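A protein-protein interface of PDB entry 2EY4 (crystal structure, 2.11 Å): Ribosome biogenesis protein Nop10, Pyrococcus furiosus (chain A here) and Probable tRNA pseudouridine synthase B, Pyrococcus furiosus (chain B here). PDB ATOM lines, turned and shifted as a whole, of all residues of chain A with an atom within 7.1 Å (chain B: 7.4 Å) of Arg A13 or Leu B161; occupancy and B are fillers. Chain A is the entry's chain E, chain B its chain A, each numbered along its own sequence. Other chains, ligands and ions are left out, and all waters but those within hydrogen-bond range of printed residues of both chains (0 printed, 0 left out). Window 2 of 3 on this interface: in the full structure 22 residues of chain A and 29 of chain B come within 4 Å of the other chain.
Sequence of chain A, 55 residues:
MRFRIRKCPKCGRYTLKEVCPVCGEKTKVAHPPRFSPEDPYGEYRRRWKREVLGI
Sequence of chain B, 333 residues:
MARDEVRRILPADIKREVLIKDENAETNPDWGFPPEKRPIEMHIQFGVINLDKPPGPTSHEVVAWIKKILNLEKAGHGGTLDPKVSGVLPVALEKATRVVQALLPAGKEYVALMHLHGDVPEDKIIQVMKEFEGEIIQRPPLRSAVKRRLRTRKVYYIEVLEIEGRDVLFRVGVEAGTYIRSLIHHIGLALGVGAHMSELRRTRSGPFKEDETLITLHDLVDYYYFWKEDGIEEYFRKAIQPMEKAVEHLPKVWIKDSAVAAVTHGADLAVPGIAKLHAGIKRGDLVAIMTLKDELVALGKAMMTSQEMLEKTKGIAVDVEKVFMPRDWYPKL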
ATOM      1  N   ARG A   6     -24.620  18.836  19.868  1.00  0.00           N
ATOM      2  CA  ARG A   6     -23.850  19.954  20.387  1.00  0.00           C
ATOM      3  C   ARG A   6     -23.720  21.040  19.329  1.00  0.00           C
ATOM      4  O   ARG A   6     -23.990  20.811  18.148  1.00  0.00           O
ATOM      5  CB  ARG A   6     -22.446  19.488  20.796  1.00  0.00           C
ATOM      6  CG  ARG A   6     -22.411  18.241  21.667  1.00  0.00           C
ATOM      7  CD  ARG A   6     -20.973  17.835  21.960  1.00  0.00           C
ATOM      8  NE  ARG A   6     -20.312  18.808  22.828  1.00  0.00           N
ATOM      9  CZ  ARG A   6     -20.400  18.805  24.155  1.00  0.00           C
ATOM     10  NH1 ARG A   6     -21.115  17.872  24.773  1.00  0.00           N
ATOM     11  NH2 ARG A   6     -19.788  19.745  24.862  1.00  0.00           N
ATOM     12  N   LYS A   7     -23.325  22.232  19.754  1.00  0.00           N
ATOM     13  CA  LYS A   7     -23.119  23.321  18.811  1.00  0.00           C
ATOM     14  C   LYS A   7     -22.008  24.206  19.340  1.00  0.00           C
ATOM     15  O   LYS A   7     -21.762  24.257  20.544  1.00  0.00           O
ATOM     16  CB  LYS A   7     -24.393  24.138  18.616  1.00  0.00           C
ATOM     17  CG  LYS A   7     -24.900  24.778  19.871  1.00  0.00           C
ATOM     18  CD  LYS A   7     -25.359  26.199  19.605  1.00  0.00           C
ATOM     19  CE  LYS A   7     -26.498  26.262  18.611  1.00  0.00           C
ATOM     20  NZ  LYS A   7     -27.036  27.647  18.567  1.00  0.00           N
ATOM     21  N   CYS A   8     -21.321  24.888  18.436  1.00  0.00           N
ATOM     22  CA  CYS A   8     -20.239  25.769  18.837  1.00  0.00           C
ATOM     23  C   CYS A   8     -20.748  27.181  19.076  1.00  0.00           C
ATOM     24  O   CYS A   8     -21.479  27.732  18.252  1.00  0.00           O
ATOM     25  CB  CYS A   8     -19.156  25.809  17.768  1.00  0.00           C
ATOM     26  SG  CYS A   8     -17.984  27.151  18.035  1.00  0.00           S
ATOM     27  N   PRO A   9     -20.361  27.786  20.211  1.00  0.00           N
ATOM     28  CA  PRO A   9     -20.772  29.145  20.575  1.00  0.00           C
ATOM     29  C   PRO A   9     -20.473  30.171  19.484  1.00  0.00           C
ATOM     30  O   PRO A   9     -21.236  31.114  19.285  1.00  0.00           O
ATOM     31  CB  PRO A   9     -19.983  29.405  21.850  1.00  0.00           C
ATOM     32  CG  PRO A   9     -19.933  28.046  22.475  1.00  0.00           C
ATOM     33  CD  PRO A   9     -19.581  27.169  21.297  1.00  0.00           C
ATOM     34  N   LYS A  10     -19.362  29.986  18.777  1.00  0.00           N
ATOM     35  CA  LYS A  10     -18.992  30.905  17.707  1.00  0.00           C
ATOM     36  C   LYS A  10     -19.122  30.208  16.354  1.00  0.00           C
ATOM     37  O   LYS A  10     -18.470  29.201  16.101  1.00  0.00           O
ATOM     38  CB  LYS A  10     -17.564  31.405  17.921  1.00  0.00           C
ATOM     39  CG  LYS A  10     -17.206  32.620  17.089  1.00  0.00           C
ATOM     40  CD  LYS A  10     -16.092  33.424  17.747  1.00  0.00           C
ATOM     41  CE  LYS A  10     -16.538  33.985  19.097  1.00  0.00           C
ATOM     42  NZ  LYS A  10     -15.482  34.802  19.765  1.00  0.00           N
ATOM     43  N   CYS A  11     -19.980  30.761  15.503  1.00  0.00           N
ATOM     44  CA  CYS A  11     -20.273  30.242  14.164  1.00  0.00           C
ATOM     45  C   CYS A  11     -21.393  29.198  14.226  1.00  0.00           C
ATOM     46  O   CYS A  11     -21.760  28.602  13.214  1.00  0.00           O
ATOM     47  CB  CYS A  11     -19.012  29.673  13.482  1.00  0.00           C
ATOM     48  SG  CYS A  11     -18.594  27.934  13.784  1.00  0.00           S
ATOM     49  N   GLY A  12     -21.932  29.006  15.429  1.00  0.00           N
ATOM     50  CA  GLY A  12     -23.036  28.084  15.672  1.00  0.00           C
ATOM     51  C   GLY A  12     -23.162  26.776  14.908  1.00  0.00           C
ATOM     52  O   GLY A  12     -24.267  26.247  14.764  1.00  0.00           O
ATOM     53  N   ARG A  13     -22.046  26.243  14.425  1.00  0.00           N
ATOM     54  CA  ARG A  13     -22.062  24.985  13.693  1.00  0.00           C
ATOM     55  C   ARG A  13     -22.563  23.874  14.613  1.00  0.00           C
ATOM     56  O   ARG A  13     -22.240  23.858  15.799  1.00  0.00           O
ATOM     57  CB  ARG A  13     -20.648  24.651  13.211  1.00  0.00           C
ATOM     58  CG  ARG A  13     -20.460  23.225  12.719  1.00  0.00           C
ATOM     59  CD  ARG A  13     -21.182  22.976  11.409  1.00  0.00           C
ATOM     60  NE  ARG A  13     -21.195  21.560  11.042  1.00  0.00           N
ATOM     61  CZ  ARG A  13     -20.108  20.825  10.824  1.00  0.00           C
ATOM     62  NH1 ARG A  13     -18.900  21.363  10.935  1.00  0.00           N
ATOM     63  NH2 ARG A  13     -20.231  19.548  10.493  1.00  0.00           N
ATOM     64  N   TYR A  14     -23.367  22.959  14.074  1.00  0.00           N
ATOM     65  CA  TYR A  14     -23.867  21.836  14.857  1.00  0.00           C
ATOM     66  C   TYR A  14     -22.964  20.625  14.644  1.00  0.00           C
ATOM     67  O   TYR A  14     -22.573  20.325  13.516  1.00  0.00           O
ATOM     68  CB  TYR A  14     -25.300  21.473  14.466  1.00  0.00           C
ATOM     69  CG  TYR A  14     -26.358  22.215  15.250  1.00  0.00           C
ATOM     70  CD1 TYR A  14     -26.886  23.419  14.786  1.00  0.00           C
ATOM     71  CD2 TYR A  14     -26.822  21.716  16.463  1.00  0.00           C
ATOM     72  CE1 TYR A  14     -27.859  24.110  15.523  1.00  0.00           C
ATOM     73  CE2 TYR A  14     -27.778  22.391  17.205  1.00  0.00           C
ATOM     74  CZ  TYR A  14     -28.294  23.590  16.729  1.00  0.00           C
ATOM     75  OH  TYR A  14     -29.223  24.266  17.485  1.00  0.00           O
ATOM     76  N   THR A  15     -22.645  19.930  15.732  1.00  0.00           N
ATOM     77  CA  THR A  15     -21.767  18.763  15.678  1.00  0.00           C
ATOM     78  C   THR A  15     -21.965  17.883  16.903  1.00  0.00           C
ATOM     79  O   THR A  15     -22.606  18.295  17.866  1.00  0.00           O
ATOM     80  CB  THR A  15     -20.279  19.194  15.634  1.00  0.00           C
ATOM     81  OG1 THR A  15     -19.435  18.043  15.759  1.00  0.00           O
ATOM     82  CG2 THR A  15     -19.971  20.150  16.774  1.00  0.00           C
ATOM     83  N   LEU A  16     -21.415  16.673  16.852  1.00  0.00           N
ATOM     84  CA  LEU A  16     -21.485  15.730  17.964  1.00  0.00           C
ATOM     85  C   LEU A  16     -20.143  15.756  18.697  1.00  0.00           C
ATOM     86  O   LEU A  16     -20.019  15.229  19.799  1.00  0.00           O
ATOM     87  CB  LEU A  16     -21.728  14.303  17.467  1.00  0.00           C
ATOM     88  CG  LEU A  16     -23.015  13.948  16.720  1.00  0.00           C
ATOM     89  CD1 LEU A  16     -22.896  12.524  16.203  1.00  0.00           C
ATOM     90  CD2 LEU A  16     -24.224  14.089  17.633  1.00  0.00           C
ATOM     91  N   LYS A  17     -19.148  16.377  18.068  1.00  0.00           N
ATOM     92  CA  LYS A  17     -17.806  16.460  18.626  1.00  0.00           C
ATOM     93  C   LYS A  17     -17.643  17.530  19.695  1.00  0.00           C
ATOM     94  O   LYS A  17     -18.248  18.603  19.615  1.00  0.00           O
ATOM     95  CB  LYS A  17     -16.801  16.683  17.496  1.00  0.00           C
ATOM     96  CG  LYS A  17     -16.793  15.541  16.485  1.00  0.00           C
ATOM     97  CD  LYS A  17     -15.780  15.753  15.376  1.00  0.00           C
ATOM     98  CE  LYS A  17     -15.762  14.571  14.410  1.00  0.00           C
ATOM     99  NZ  LYS A  17     -17.078  14.374  13.721  1.00  0.00           N
ATOM    100  N   CYS A  20     -15.263  21.976  18.054  1.00  0.00           N
ATOM    101  CA  CYS A  20     -15.779  22.307  16.732  1.00  0.00           C
ATOM    102  C   CYS A  20     -14.763  22.040  15.637  1.00  0.00           C
ATOM    103  O   CYS A  20     -13.604  22.437  15.743  1.00  0.00           O
ATOM    104  CB  CYS A  20     -16.202  23.770  16.653  1.00  0.00           C
ATOM    105  SG  CYS A  20     -16.666  24.228  14.971  1.00  0.00           S
ATOM    106  N   PRO A  21     -15.191  21.365  14.564  1.00  0.00           N
ATOM    107  CA  PRO A  21     -14.302  21.049  13.444  1.00  0.00           C
ATOM    108  C   PRO A  21     -13.922  22.293  12.644  1.00  0.00           C
ATOM    109  O   PRO A  21     -12.903  22.316  11.951  1.00  0.00           O
ATOM    110  CB  PRO A  21     -15.131  20.072  12.610  1.00  0.00           C
ATOM    111  CG  PRO A  21     -16.082  19.466  13.610  1.00  0.00           C
ATOM    112  CD  PRO A  21     -16.478  20.663  14.426  1.00  0.00           C
ATOM    113  N   VAL A  22     -14.747  23.328  12.755  1.00  0.00           N
ATOM    114  CA  VAL A  22     -14.529  24.565  12.016  1.00  0.00           C
ATOM    115  C   VAL A  22     -13.590  25.573  12.677  1.00  0.00           C
ATOM    116  O   VAL A  22     -12.644  26.042  12.042  1.00  0.00           O
ATOM    117  CB  VAL A  22     -15.878  25.266  11.722  1.00  0.00           C
ATOM    118  CG1 VAL A  22     -15.655  26.485  10.843  1.00  0.00           C
ATOM    119  CG2 VAL A  22     -16.831  24.293  11.048  1.00  0.00           C
ATOM    120  N   CYS A  23     -13.840  25.909  13.940  1.00  0.00           N
ATOM    121  CA  CYS A  23     -13.006  26.889  14.634  1.00  0.00           C
ATOM    122  C   CYS A  23     -12.149  26.340  15.772  1.00  0.00           C
ATOM    123  O   CYS A  23     -11.364  27.076  16.371  1.00  0.00           O
ATOM    124  CB  CYS A  23     -13.875  28.031  15.167  1.00  0.00           C
ATOM    125  SG  CYS A  23     -15.032  27.542  16.455  1.00  0.00           S
ATOM    126  N   THR A  27     -17.276  22.964  22.118  1.00  0.00           N
ATOM    127  CA  THR A  27     -18.722  22.980  21.913  1.00  0.00           C
ATOM    128  C   THR A  27     -19.502  22.621  23.180  1.00  0.00           C
ATOM    129  O   THR A  27     -18.943  22.118  24.159  1.00  0.00           O
ATOM    130  CB  THR A  27     -19.141  22.006  20.781  1.00  0.00           C
ATOM    131  OG1 THR A  27     -18.839  20.654  21.157  1.00  0.00           O
ATOM    132  CG2 THR A  27     -18.413  22.345  19.497  1.00  0.00           C
ATOM    133  N   TYR B 110     -34.981  21.440  11.353  1.00  0.00           N
ATOM    134  CA  TYR B 110     -34.540  20.706  12.515  1.00  0.00           C
ATOM    135  C   TYR B 110     -33.121  20.209  12.333  1.00  0.00           C
ATOM    136  O   TYR B 110     -32.603  20.180  11.227  1.00  0.00           O
ATOM    137  CB  TYR B 110     -35.427  19.478  12.749  1.00  0.00           C
ATOM    138  CG  TYR B 110     -36.874  19.764  13.055  1.00  0.00           C
ATOM    139  CD1 TYR B 110     -37.805  19.956  12.034  1.00  0.00           C
ATOM    140  CD2 TYR B 110     -37.312  19.859  14.371  1.00  0.00           C
ATOM    141  CE1 TYR B 110     -39.141  20.238  12.326  1.00  0.00           C
ATOM    142  CE2 TYR B 110     -38.635  20.138  14.671  1.00  0.00           C
ATOM    143  CZ  TYR B 110     -39.544  20.330  13.649  1.00  0.00           C
ATOM    144  OH  TYR B 110     -40.843  20.641  13.973  1.00  0.00           O
ATOM    145  N   VAL B 111     -32.499  19.841  13.445  1.00  0.00           N
ATOM    146  CA  VAL B 111     -31.188  19.223  13.442  1.00  0.00           C
ATOM    147  C   VAL B 111     -31.536  17.940  14.191  1.00  0.00           C
ATOM    148  O   VAL B 111     -31.957  17.976  15.350  1.00  0.00           O
ATOM    149  CB  VAL B 111     -30.135  20.020  14.226  1.00  0.00           C
ATOM    150  CG1 VAL B 111     -28.933  19.118  14.515  1.00  0.00           C
ATOM    151  CG2 VAL B 111     -29.692  21.240  13.416  1.00  0.00           C
ATOM    152  N   ALA B 112     -31.388  16.809  13.516  1.00  0.00           N
ATOM    153  CA  ALA B 112     -31.745  15.539  14.112  1.00  0.00           C
ATOM    154  C   ALA B 112     -30.615  14.525  14.155  1.00  0.00           C
ATOM    155  O   ALA B 112     -29.680  14.562  13.348  1.00  0.00           O
ATOM    156  CB  ALA B 112     -32.942  14.944  13.363  1.00  0.00           C
ATOM    157  N   GLU B 122     -21.161   5.071   4.420  1.00  0.00           N
ATOM    158  CA  GLU B 122     -21.546   6.475   4.373  1.00  0.00           C
ATOM    159  C   GLU B 122     -22.185   6.887   3.053  1.00  0.00           C
ATOM    160  O   GLU B 122     -23.277   7.464   3.031  1.00  0.00           O
ATOM    161  CB  GLU B 122     -20.321   7.345   4.658  1.00  0.00           C
ATOM    162  CG  GLU B 122     -20.627   8.818   4.844  1.00  0.00           C
ATOM    163  CD  GLU B 122     -19.448   9.586   5.406  1.00  0.00           C
ATOM    164  OE1 GLU B 122     -19.583  10.806   5.635  1.00  0.00           O
ATOM    165  OE2 GLU B 122     -18.386   8.965   5.618  1.00  0.00           O
ATOM    166  N   ILE B 158     -32.218  18.087   2.895  1.00  0.00           N
ATOM    167  CA  ILE B 158     -31.645  17.196   3.887  1.00  0.00           C
ATOM    168  C   ILE B 158     -30.133  17.323   3.742  1.00  0.00           C
ATOM    169  O   ILE B 158     -29.586  17.117   2.657  1.00  0.00           O
ATOM    170  CB  ILE B 158     -32.060  15.728   3.653  1.00  0.00           C
ATOM    171  CG1 ILE B 158     -33.563  15.573   3.883  1.00  0.00           C
ATOM    172  CG2 ILE B 158     -31.308  14.819   4.600  1.00  0.00           C
ATOM    173  CD1 ILE B 158     -34.059  14.148   3.795  1.00  0.00           C
ATOM    174  N   GLU B 159     -29.471  17.691   4.834  1.00  0.00           N
ATOM    175  CA  GLU B 159     -28.025  17.867   4.843  1.00  0.00           C
ATOM    176  C   GLU B 159     -27.385  17.074   5.984  1.00  0.00           C
ATOM    177  O   GLU B 159     -27.590  17.385   7.157  1.00  0.00           O
ATOM    178  CB  GLU B 159     -27.695  19.353   4.989  1.00  0.00           C
ATOM    179  CG  GLU B 159     -26.214  19.674   5.018  1.00  0.00           C
ATOM    180  CD  GLU B 159     -25.945  21.161   5.156  1.00  0.00           C
ATOM    181  OE1 GLU B 159     -26.420  21.759   6.145  1.00  0.00           O
ATOM    182  OE2 GLU B 159     -25.259  21.728   4.279  1.00  0.00           O
ATOM    183  N   VAL B 160     -26.618  16.044   5.634  1.00  0.00           N
ATOM    184  CA  VAL B 160     -25.954  15.223   6.637  1.00  0.00           C
ATOM    185  C   VAL B 160     -24.787  16.034   7.185  1.00  0.00           C
ATOM    186  O   VAL B 160     -23.970  16.547   6.423  1.00  0.00           O
ATOM    187  CB  VAL B 160     -25.434  13.901   6.028  1.00  0.00           C
ATOM    188  CG1 VAL B 160     -24.605  13.143   7.051  1.00  0.00           C
ATOM    189  CG2 VAL B 160     -26.607  13.049   5.576  1.00  0.00           C
ATOM    190  N   LEU B 161     -24.718  16.157   8.508  1.00  0.00           N
ATOM    191  CA  LEU B 161     -23.668  16.940   9.144  1.00  0.00           C
ATOM    192  C   LEU B 161     -22.467  16.114   9.575  1.00  0.00           C
ATOM    193  O   LEU B 161     -21.337  16.410   9.199  1.00  0.00           O
ATOM    194  CB  LEU B 161     -24.233  17.688  10.354  1.00  0.00           C
ATOM    195  CG  LEU B 161     -25.360  18.685  10.055  1.00  0.00           C
ATOM    196  CD1 LEU B 161     -25.921  19.202  11.362  1.00  0.00           C
ATOM    197  CD2 LEU B 161     -24.837  19.842   9.205  1.00  0.00           C
ATOM    198  N   GLU B 162     -22.712  15.081  10.366  1.00  0.00           N
ATOM    199  CA  GLU B 162     -21.630  14.241  10.846  1.00  0.00           C
ATOM    200  C   GLU B 162     -22.080  12.815  11.058  1.00  0.00           C
ATOM    201  O   GLU B 162     -23.243  12.554  11.356  1.00  0.00           O
ATOM    202  CB  GLU B 162     -21.073  14.798  12.156  1.00  0.00           C
ATOM    203  CG  GLU B 162     -20.072  15.912  11.963  1.00  0.00           C
ATOM    204  CD  GLU B 162     -19.732  16.633  13.256  1.00  0.00           C
ATOM    205  OE1 GLU B 162     -19.577  15.963  14.301  1.00  0.00           O
ATOM    206  OE2 GLU B 162     -19.608  17.876  13.217  1.00  0.00           O
ATOM    207  N   ILE B 163     -21.139  11.894  10.904  1.00  0.00           N
ATOM    208  CA  ILE B 163     -21.423  10.480  11.088  1.00  0.00           C
ATOM    209  C   ILE B 163     -20.422   9.875  12.060  1.00  0.00           C
ATOM    210  O   ILE B 163     -19.221   9.881  11.810  1.00  0.00           O
ATOM    211  CB  ILE B 163     -21.353   9.718   9.749  1.00  0.00           C
ATOM    212  CG1 ILE B 163     -22.337  10.336   8.754  1.00  0.00           C
ATOM    213  CG2 ILE B 163     -21.665   8.248   9.967  1.00  0.00           C
ATOM    214  CD1 ILE B 163     -22.461   9.591   7.449  1.00  0.00           C
ATOM    215  N   VAL B 168     -26.055   9.266  13.015  1.00  0.00           N
ATOM    216  CA  VAL B 168     -26.040  10.195  11.897  1.00  0.00           C
ATOM    217  C   VAL B 168     -26.717  11.512  12.264  1.00  0.00           C
ATOM    218  O   VAL B 168     -27.919  11.552  12.533  1.00  0.00           O
ATOM    219  CB  VAL B 168     -26.761   9.586  10.683  1.00  0.00           C
ATOM    220  CG1 VAL B 168     -26.680  10.531   9.485  1.00  0.00           C
ATOM    221  CG2 VAL B 168     -26.151   8.235  10.356  1.00  0.00           C
ATOM    222  N   LEU B 169     -25.936  12.587  12.276  1.00  0.00           N
ATOM    223  CA  LEU B 169     -26.467  13.907  12.591  1.00  0.00           C
ATOM    224  C   LEU B 169     -26.758  14.623  11.276  1.00  0.00           C
ATOM    225  O   LEU B 169     -25.909  14.659  10.384  1.00  0.00           O
ATOM    226  CB  LEU B 169     -25.450  14.705  13.415  1.00  0.00           C
ATOM    227  CG  LEU B 169     -25.895  16.093  13.895  1.00  0.00           C
ATOM    228  CD1 LEU B 169     -27.174  15.988  14.731  1.00  0.00           C
ATOM    229  CD2 LEU B 169     -24.789  16.727  14.707  1.00  0.00           C
ATOM    230  N   PHE B 170     -27.956  15.183  11.145  1.00  0.00           N
ATOM    231  CA  PHE B 170     -28.324  15.886   9.919  1.00  0.00           C
ATOM    232  C   PHE B 170     -29.285  17.045  10.147  1.00  0.00           C
ATOM    233  O   PHE B 170     -30.016  17.072  11.132  1.00  0.00           O
ATOM    234  CB  PHE B 170     -28.951  14.908   8.930  1.00  0.00           C
ATOM    235  CG  PHE B 170     -30.302  14.390   9.350  1.00  0.00           C
ATOM    236  CD1 PHE B 170     -31.472  14.999   8.895  1.00  0.00           C
ATOM    237  CD2 PHE B 170     -30.408  13.255  10.154  1.00  0.00           C
ATOM    238  CE1 PHE B 170     -32.725  14.483   9.231  1.00  0.00           C
ATOM    239  CE2 PHE B 170     -31.652  12.730  10.498  1.00  0.00           C
ATOM    240  CZ  PHE B 170     -32.815  13.340  10.031  1.00  0.00           C
ATOM    241  N   ARG B 171     -29.271  18.003   9.226  1.00  0.00           N
ATOM    242  CA  ARG B 171     -30.151  19.164   9.295  1.00  0.00           C
ATOM    243  C   ARG B 171     -31.238  18.930   8.254  1.00  0.00           C
ATOM    244  O   ARG B 171     -30.948  18.498   7.135  1.00  0.00           O
ATOM    245  CB  ARG B 171     -29.389  20.441   8.947  1.00  0.00           C
ATOM    246  CG  ARG B 171     -30.175  21.731   9.170  1.00  0.00           C
ATOM    247  CD  ARG B 171     -29.545  22.886   8.396  1.00  0.00           C
ATOM    248  NE  ARG B 171     -28.090  22.891   8.516  1.00  0.00           N
ATOM    249  CZ  ARG B 171     -27.431  23.127   9.648  1.00  0.00           C
ATOM    250  NH1 ARG B 171     -28.099  23.389  10.766  1.00  0.00           N
ATOM    251  NH2 ARG B 171     -26.105  23.085   9.667  1.00  0.00           N
ATOM    252  N   VAL B 172     -32.485  19.218   8.607  1.00  0.00           N
ATOM    253  CA  VAL B 172     -33.577  19.001   7.668  1.00  0.00           C
ATOM    254  C   VAL B 172     -34.614  20.130   7.676  1.00  0.00           C
ATOM    255  O   VAL B 172     -35.060  20.558   8.738  1.00  0.00           O
ATOM    256  CB  VAL B 172     -34.251  17.633   7.964  1.00  0.00           C
ATOM    257  CG1 VAL B 172     -34.942  17.670   9.319  1.00  0.00           C
ATOM    258  CG2 VAL B 172     -35.219  17.269   6.855  1.00  0.00           C
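Gly A12 touches none of the printed residues of chain B.
Of the printed residues of chain B, Tyr A14 touches Val B111, Leu B161 and Glu B162.
Of the printed residues of chain B, Lys A17 touches Glu B162 (3.0 Å).
Printed residues of chain B within 4 Å of Pro A21: Glu B162.
Cys A23 touches none of the printed residues of chain B.
Leu B161 touches just these residues of chain A: Arg A13 and Tyr A14.
Of the printed residues of chain A, Glu B162 touches Arg A13, Tyr A14, Thr A15, Leu A16, Lys A17 and Pro A21.
The nearest residue of chain A that does not touch Leu B161 is Thr A15 (5.5 Å).
The nearest printed residue of chain A that does not touch Leu B169 is Tyr A14 (4.3 Å).
Of the 15 printed residues of chain B, 4 touch a printed residue of chain A.
Hydrophobic or aromatic side chains of chain A within 4 Å of the printed part of chain B: Tyr A14, Leu A16 and Pro A21.
Among the printed residues, Asp or Glu carboxylates within 4 Å of a Lys or Arg side-chain nitrogen of the other chain: Arg A13 with Glu B162 and Lys A17 with Glu B162.
The side-chain carboxylate of Glu B162 is in salt-bridge range of the guanidinium group of Arg A13 (3.3 Å).
OG1 of Thr A15 lies within hydrogen-bond range of OE1 of Glu B162, at 2.5 Å.
The side-chain carboxylate of Glu B162 lies within hydrogen-bond range of the backbone NH of Leu A16.
OE1 of Glu B162 lies within salt-bridge range of NZ of Lys A17 (3.0 Å).
N of Leu B161 sits at hydrogen-bond distance from O of Leu B169, 2.7 Å away.
The backbone NH (N) of Leu B169 sits at hydrogen-bond distance from the backbone carbonyl oxygen (O) of Glu B162, at 2.8 Å.
The backbone NH of Arg A6 lies within hydrogen-bond range of the backbone carbonyl oxygen of Thr A15, 2.9 Å away.
The backbone carbonyl oxygen (O) of Arg A13 lies within hydrogen-bond range of the backbone NH (N) of Cys A8 (3.0 Å).
The side-chain hydroxyl of Thr A15 sits at hydrogen-bond distance from the backbone NH of Lys A17 (2.9 Å).
O of Lys A17 lies within hydrogen-bond range of OG1 of Thr A27 (2.6 Å).
Among the printed residues, merely in contact across the chains: Arg A13 with Leu B161 (3.6 Å), Tyr A14 with Val B111 (3.8 Å), Tyr A14 with Leu B161 (3.9 Å), Tyr A14 with Glu B162 (3.9 Å), Thr A15 with Leu B169 (3.8 Å), Leu A16 with Leu B169 (3.9 Å) and Pro A21 with Glu B162 (3.9 Å).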
